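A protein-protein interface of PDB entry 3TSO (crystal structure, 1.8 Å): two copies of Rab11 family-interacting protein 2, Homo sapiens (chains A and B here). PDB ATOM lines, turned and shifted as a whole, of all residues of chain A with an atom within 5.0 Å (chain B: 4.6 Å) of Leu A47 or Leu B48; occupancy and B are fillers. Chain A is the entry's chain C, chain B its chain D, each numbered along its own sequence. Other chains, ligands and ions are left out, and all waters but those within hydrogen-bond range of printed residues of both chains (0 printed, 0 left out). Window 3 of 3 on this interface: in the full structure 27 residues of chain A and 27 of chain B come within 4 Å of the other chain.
The backbone carbonyl oxygen (O) of Ile B58 lies within hydrogen-bond range of the guanidinium group (NH1) of Arg A50, at 2.8 Å.
Tyr A43 touches Ile B44. Tyr A43 touches Leu B48. CG1 of Ile A44 touches CG1 of Ile B44 (3.4 Å). Leu B47 touches Leu A47. Leu B48 touches Leu A47 (CD2 to CD2, 3.8 Å). Leu A47 touches Ile B58. Leu B47 touches Leu A48. Val A51 touches Val B51 (CG2 to CG2, 3.8 Å). Ile B58 touches Val A51.
Ile A44 touches its own counterpart, Ile B44. Leu A47 touches its own counterpart, Leu B47. Leu A47 touches Leu B48, and with the chains exchanged Leu A48 touches Leu B47. Val A51 touches its own counterpart, Val B51. 8 positions are printed for both chains.
Hydrophobic or aromatic side chains of chain B within 4 Å of the printed part of chain A: Ile B44, Leu B47, Leu B48, Val B51 and Ile B58. Of the 10 printed residues of chain A, 6 touch a printed residue of chain B. Among the printed residues, 10 pairs touch across the chains.
Leu A47 touches just these residues of chain B: Leu B47, Leu B48 and Ile B58. Of chain A, only Tyr A43 (3.7 Å) and Leu A47 (3.8 Å) come within 4 Å of Leu B48. Printed residues of chain A within 4 Å of Leu B47: Leu A47 (3.6 Å) and Leu A48 (3.8 Å). Of the printed residues of chain B, Leu A48 touches Leu B47 (3.8 Å). Asn B46 touches none of the printed residues of chain A. The nearest residue of chain B that does not touch Leu A47 is Leu B59 (4.1 Å).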
ATOM      1  N   ASP A  42      37.230   6.700  -3.282  1.00  0.00           N
ATOM      2  CA  ASP A  42      37.035   8.146  -3.469  1.00  0.00           C
ATOM      3  C   ASP A  42      36.271   8.480  -4.769  1.00  0.00           C
ATOM      4  O   ASP A  42      35.319   9.259  -4.750  1.00  0.00           O
ATOM      5  CB  ASP A  42      38.349   8.919  -3.459  1.00  0.00           C
ATOM      6  CG  ASP A  42      38.980   9.063  -2.052  1.00  0.00           C
ATOM      7  OD1 ASP A  42      38.378   8.676  -1.032  1.00  0.00           O
ATOM      8  OD2 ASP A  42      40.127   9.584  -2.034  1.00  0.00           O
ATOM      9  N   TYR A  43      36.598   7.816  -5.896  1.00  0.00           N
ATOM     10  CA  TYR A  43      35.801   8.012  -7.080  1.00  0.00           C
ATOM     11  C   TYR A  43      34.293   7.699  -6.782  1.00  0.00           C
ATOM     12  O   TYR A  43      33.385   8.510  -7.095  1.00  0.00           O
ATOM     13  CB  TYR A  43      36.319   7.103  -8.219  1.00  0.00           C
ATOM     14  CG  TYR A  43      35.506   7.251  -9.458  1.00  0.00           C
ATOM     15  CD1 TYR A  43      34.469   6.349  -9.726  1.00  0.00           C
ATOM     16  CD2 TYR A  43      35.732   8.373 -10.344  1.00  0.00           C
ATOM     17  CE1 TYR A  43      33.648   6.530 -10.875  1.00  0.00           C
ATOM     18  CE2 TYR A  43      34.993   8.550 -11.454  1.00  0.00           C
ATOM     19  CZ  TYR A  43      33.932   7.596 -11.753  1.00  0.00           C
ATOM     20  OH  TYR A  43      33.122   7.795 -12.875  1.00  0.00           O
ATOM     21  N   ILE A  44      34.041   6.534  -6.208  1.00  0.00           N
ATOM     22  CA  ILE A  44      32.691   6.095  -5.917  1.00  0.00           C
ATOM     23  C   ILE A  44      31.957   7.173  -5.059  1.00  0.00           C
ATOM     24  O   ILE A  44      30.776   7.559  -5.310  1.00  0.00           O
ATOM     25  CB  ILE A  44      32.748   4.720  -5.193  1.00  0.00           C
ATOM     26  CG1 ILE A  44      33.158   3.649  -6.182  1.00  0.00           C
ATOM     27  CG2 ILE A  44      31.359   4.344  -4.499  1.00  0.00           C
ATOM     28  CD1 ILE A  44      33.489   2.259  -5.528  1.00  0.00           C
ATOM     29  N   ASP A  45      32.618   7.600  -4.010  1.00  0.00           N
ATOM     30  CA  ASP A  45      32.006   8.557  -3.107  1.00  0.00           C
ATOM     31  C   ASP A  45      31.672   9.883  -3.788  1.00  0.00           C
ATOM     32  O   ASP A  45      30.553  10.414  -3.654  1.00  0.00           O
ATOM     33  CB  ASP A  45      32.916   8.722  -1.891  1.00  0.00           C
ATOM     34  CG  ASP A  45      32.742   7.586  -0.916  1.00  0.00           C
ATOM     35  OD1 ASP A  45      31.809   6.737  -1.077  1.00  0.00           O
ATOM     36  OD2 ASP A  45      33.562   7.486  -0.028  1.00  0.00           O
ATOM     37  N   ASN A  46      32.616  10.387  -4.584  1.00  0.00           N
ATOM     38  CA  ASN A  46      32.379  11.637  -5.311  1.00  0.00           C
ATOM     39  C   ASN A  46      31.238  11.468  -6.287  1.00  0.00           C
ATOM     40  O   ASN A  46      30.385  12.340  -6.382  1.00  0.00           O
ATOM     41  CB  ASN A  46      33.643  12.092  -6.036  1.00  0.00           C
ATOM     42  CG  ASN A  46      34.708  12.543  -5.087  1.00  0.00           C
ATOM     43  OD1 ASN A  46      34.397  12.965  -3.994  1.00  0.00           O
ATOM     44  ND2 ASN A  46      35.967  12.531  -5.520  1.00  0.00           N
ATOM     45  N   LEU A  47      31.247  10.385  -7.076  1.00  0.00           N
ATOM     46  CA  LEU A  47      30.112  10.058  -7.962  1.00  0.00           C
ATOM     47  C   LEU A  47      28.734   9.936  -7.213  1.00  0.00           C
ATOM     48  O   LEU A  47      27.691  10.484  -7.683  1.00  0.00           O
ATOM     49  CB  LEU A  47      30.388   8.713  -8.692  1.00  0.00           C
ATOM     50  CG  LEU A  47      29.267   8.230  -9.645  1.00  0.00           C
ATOM     51  CD1 LEU A  47      28.876   9.283 -10.696  1.00  0.00           C
ATOM     52  CD2 LEU A  47      29.729   6.940 -10.366  1.00  0.00           C
ATOM     53  N   LEU A  48      28.707   9.215  -6.090  1.00  0.00           N
ATOM     54  CA  LEU A  48      27.450   9.007  -5.331  1.00  0.00           C
ATOM     55  C   LEU A  48      26.876  10.348  -4.771  1.00  0.00           C
ATOM     56  O   LEU A  48      25.641  10.490  -4.580  1.00  0.00           O
ATOM     57  CB  LEU A  48      27.732   8.041  -4.170  1.00  0.00           C
ATOM     58  CG  LEU A  48      27.749   6.529  -4.583  1.00  0.00           C
ATOM     59  CD1 LEU A  48      28.164   5.600  -3.436  1.00  0.00           C
ATOM     60  CD2 LEU A  48      26.432   6.032  -5.173  1.00  0.00           C
ATOM     61  N   VAL A  49      27.747  11.314  -4.521  1.00  0.00           N
ATOM     62  CA  VAL A  49      27.264  12.635  -4.007  1.00  0.00           C
ATOM     63  C   VAL A  49      26.375  13.210  -5.117  1.00  0.00           C
ATOM     64  O   VAL A  49      25.286  13.766  -4.829  1.00  0.00           O
ATOM     65  CB  VAL A  49      28.437  13.622  -3.623  1.00  0.00           C
ATOM     66  CG1 VAL A  49      27.955  15.110  -3.564  1.00  0.00           C
ATOM     67  CG2 VAL A  49      29.069  13.244  -2.220  1.00  0.00           C
ATOM     68  N   ARG A  50      26.838  13.080  -6.375  1.00  0.00           N
ATOM     69  CA  ARG A  50      26.142  13.670  -7.484  1.00  0.00           C
ATOM     70  C   ARG A  50      24.866  12.863  -7.685  1.00  0.00           C
ATOM     71  O   ARG A  50      23.826  13.450  -7.878  1.00  0.00           O
ATOM     72  CB  ARG A  50      26.994  13.702  -8.781  1.00  0.00           C
ATOM     73  CG  ARG A  50      28.288  14.504  -8.662  1.00  0.00           C
ATOM     74  CD  ARG A  50      29.137  14.400  -9.931  1.00  0.00           C
ATOM     75  NE  ARG A  50      30.437  15.082  -9.811  1.00  0.00           N
ATOM     76  CZ  ARG A  50      31.287  15.287 -10.825  1.00  0.00           C
ATOM     77  NH1 ARG A  50      30.996  14.861 -12.060  1.00  0.00           N
ATOM     78  NH2 ARG A  50      32.434  15.922 -10.612  1.00  0.00           N
ATOM     79  N   VAL A  51      24.943  11.524  -7.647  1.00  0.00           N
ATOM     80  CA  VAL A  51      23.800  10.701  -7.839  1.00  0.00           C
ATOM     81  C   VAL A  51      22.754  10.996  -6.787  1.00  0.00           C
ATOM     82  O   VAL A  51      21.562  11.152  -7.149  1.00  0.00           O
ATOM     83  CB  VAL A  51      24.162   9.152  -7.881  1.00  0.00           C
ATOM     84  CG1 VAL A  51      22.897   8.295  -7.897  1.00  0.00           C
ATOM     85  CG2 VAL A  51      25.007   8.808  -9.107  1.00  0.00           C
ATOM     86  N   ILE B  44      31.465   0.106  -9.745  1.00  0.00           N
ATOM     87  CA  ILE B  44      31.560   1.295 -10.540  1.00  0.00           C
ATOM     88  C   ILE B  44      30.927   1.139 -11.909  1.00  0.00           C
ATOM     89  O   ILE B  44      30.113   1.989 -12.344  1.00  0.00           O
ATOM     90  CB  ILE B  44      33.067   1.755 -10.654  1.00  0.00           C
ATOM     91  CG1 ILE B  44      33.523   2.334  -9.276  1.00  0.00           C
ATOM     92  CG2 ILE B  44      33.201   2.824 -11.754  1.00  0.00           C
ATOM     93  CD1 ILE B  44      35.085   2.517  -9.178  1.00  0.00           C
ATOM     94  N   ASP B  45      31.191   0.001 -12.558  1.00  0.00           N
ATOM     95  CA  ASP B  45      30.714  -0.211 -13.910  1.00  0.00           C
ATOM     96  C   ASP B  45      29.199  -0.342 -13.902  1.00  0.00           C
ATOM     97  O   ASP B  45      28.506   0.230 -14.748  1.00  0.00           O
ATOM     98  CB  ASP B  45      31.369  -1.482 -14.542  1.00  0.00           C
ATOM     99  CG  ASP B  45      32.826  -1.225 -14.934  1.00  0.00           C
ATOM    100  OD1 ASP B  45      33.220  -0.018 -15.056  1.00  0.00           O
ATOM    101  OD2 ASP B  45      33.568  -2.219 -15.104  1.00  0.00           O
ATOM    102  N   ASN B  46      28.698  -1.086 -12.919  1.00  0.00           N
ATOM    103  CA  ASN B  46      27.264  -1.273 -12.852  1.00  0.00           C
ATOM    104  C   ASN B  46      26.548   0.045 -12.552  1.00  0.00           C
ATOM    105  O   ASN B  46      25.556   0.335 -13.204  1.00  0.00           O
ATOM    106  CB  ASN B  46      26.865  -2.386 -11.876  1.00  0.00           C
ATOM    107  CG  ASN B  46      27.334  -3.769 -12.357  1.00  0.00           C
ATOM    108  OD1 ASN B  46      27.446  -4.014 -13.559  1.00  0.00           O
ATOM    109  ND2 ASN B  46      27.677  -4.621 -11.435  1.00  0.00           N
ATOM    110  N   LEU B  47      27.057   0.832 -11.605  1.00  0.00           N
ATOM    111  CA  LEU B  47      26.499   2.170 -11.366  1.00  0.00           C
ATOM    112  C   LEU B  47      26.549   3.126 -12.553  1.00  0.00           C
ATOM    113  O   LEU B  47      25.567   3.870 -12.815  1.00  0.00           O
ATOM    114  CB  LEU B  47      27.158   2.850 -10.170  1.00  0.00           C
ATOM    115  CG  LEU B  47      26.722   4.257  -9.740  1.00  0.00           C
ATOM    116  CD1 LEU B  47      25.183   4.219  -9.389  1.00  0.00           C
ATOM    117  CD2 LEU B  47      27.575   4.698  -8.551  1.00  0.00           C
ATOM    118  N   LEU B  48      27.691   3.135 -13.244  1.00  0.00           N
ATOM    119  CA  LEU B  48      27.824   4.015 -14.393  1.00  0.00           C
ATOM    120  C   LEU B  48      26.830   3.642 -15.507  1.00  0.00           C
ATOM    121  O   LEU B  48      26.402   4.489 -16.284  1.00  0.00           O
ATOM    122  CB  LEU B  48      29.262   3.904 -14.933  1.00  0.00           C
ATOM    123  CG  LEU B  48      30.272   4.731 -14.108  1.00  0.00           C
ATOM    124  CD1 LEU B  48      31.681   4.487 -14.634  1.00  0.00           C
ATOM    125  CD2 LEU B  48      29.954   6.272 -14.090  1.00  0.00           C
ATOM    126  N   VAL B  49      26.497   2.375 -15.621  1.00  0.00           N
ATOM    127  CA  VAL B  49      25.550   1.982 -16.661  1.00  0.00           C
ATOM    128  C   VAL B  49      24.243   2.724 -16.415  1.00  0.00           C
ATOM    129  O   VAL B  49      23.632   3.256 -17.350  1.00  0.00           O
ATOM    130  CB  VAL B  49      25.267   0.506 -16.632  1.00  0.00           C
ATOM    131  CG1 VAL B  49      23.888   0.167 -17.225  1.00  0.00           C
ATOM    132  CG2 VAL B  49      26.402  -0.281 -17.353  1.00  0.00           C
ATOM    133  N   ARG B  50      23.810   2.717 -15.181  1.00  0.00           N
ATOM    134  CA  ARG B  50      22.589   3.383 -14.820  1.00  0.00           C
ATOM    135  C   ARG B  50      22.703   4.885 -14.945  1.00  0.00           C
ATOM    136  O   ARG B  50      21.810   5.486 -15.399  1.00  0.00           O
ATOM    137  CB  ARG B  50      22.100   2.987 -13.433  1.00  0.00           C
ATOM    138  CG  ARG B  50      21.969   1.526 -13.196  1.00  0.00           C
ATOM    139  N   VAL B  51      23.818   5.469 -14.552  1.00  0.00           N
ATOM    140  CA  VAL B  51      24.010   6.892 -14.676  1.00  0.00           C
ATOM    141  C   VAL B  51      23.983   7.289 -16.159  1.00  0.00           C
ATOM    142  O   VAL B  51      23.421   8.263 -16.534  1.00  0.00           O
ATOM    143  CB  VAL B  51      25.319   7.356 -14.024  1.00  0.00           C
ATOM    144  CG1 VAL B  51      25.606   8.781 -14.329  1.00  0.00           C
ATOM    145  CG2 VAL B  51      25.288   7.142 -12.564  1.00  0.00           C
ATOM    146  N   MET B  52      24.648   6.508 -16.973  1.00  0.00           N
ATOM    147  CA  MET B  52      24.742   6.810 -18.377  1.00  0.00           C
ATOM    148  C   MET B  52      23.363   6.724 -19.029  1.00  0.00           C
ATOM    149  O   MET B  52      23.110   7.373 -19.975  1.00  0.00           O
ATOM    150  CB  MET B  52      25.752   5.891 -19.079  1.00  0.00           C
ATOM    151  CG  MET B  52      27.207   6.224 -18.822  1.00  0.00           C
ATOM    152  SD  MET B  52      28.446   5.082 -19.458  1.00  0.00           S
ATOM    153  CE  MET B  52      28.548   5.701 -21.008  1.00  0.00           C
ATOM    154  N   ILE B  58      25.823  13.948 -15.234  1.00  0.00           N
ATOM    155  CA  ILE B  58      26.624  13.685 -14.027  1.00  0.00           C
ATOM    156  C   ILE B  58      28.075  13.401 -14.381  1.00  0.00           C
ATOM    157  O   ILE B  58      28.986  13.706 -13.598  1.00  0.00           O
ATOM    158  CB  ILE B  58      25.943  12.543 -13.177  1.00  0.00           C
ATOM    159  CG1 ILE B  58      24.766  13.129 -12.401  1.00  0.00           C
ATOM    160  CG2 ILE B  58      26.958  11.799 -12.260  1.00  0.00           C
ATOM    161  CD1 ILE B  58      24.059  12.078 -11.488  1.00  0.00           C
ATOM    162  N   LEU B  59      28.312  12.852 -15.565  1.00  0.00           N
ATOM    163  CA  LEU B  59      29.692  12.467 -15.919  1.00  0.00           C
ATOM    164  C   LEU B  59      30.495  13.608 -16.654  1.00  0.00           C
ATOM    165  O   LEU B  59      31.649  13.417 -17.079  1.00  0.00           O
ATOM    166  CB  LEU B  59      29.563  11.222 -16.753  1.00  0.00           C
ATOM    167  CG  LEU B  59      28.759  10.113 -15.985  1.00  0.00           C
ATOM    168  CD1 LEU B  59      28.797   8.893 -16.951  1.00  0.00           C
ATOM    169  CD2 LEU B  59      29.482   9.727 -14.698  1.00  0.00           C
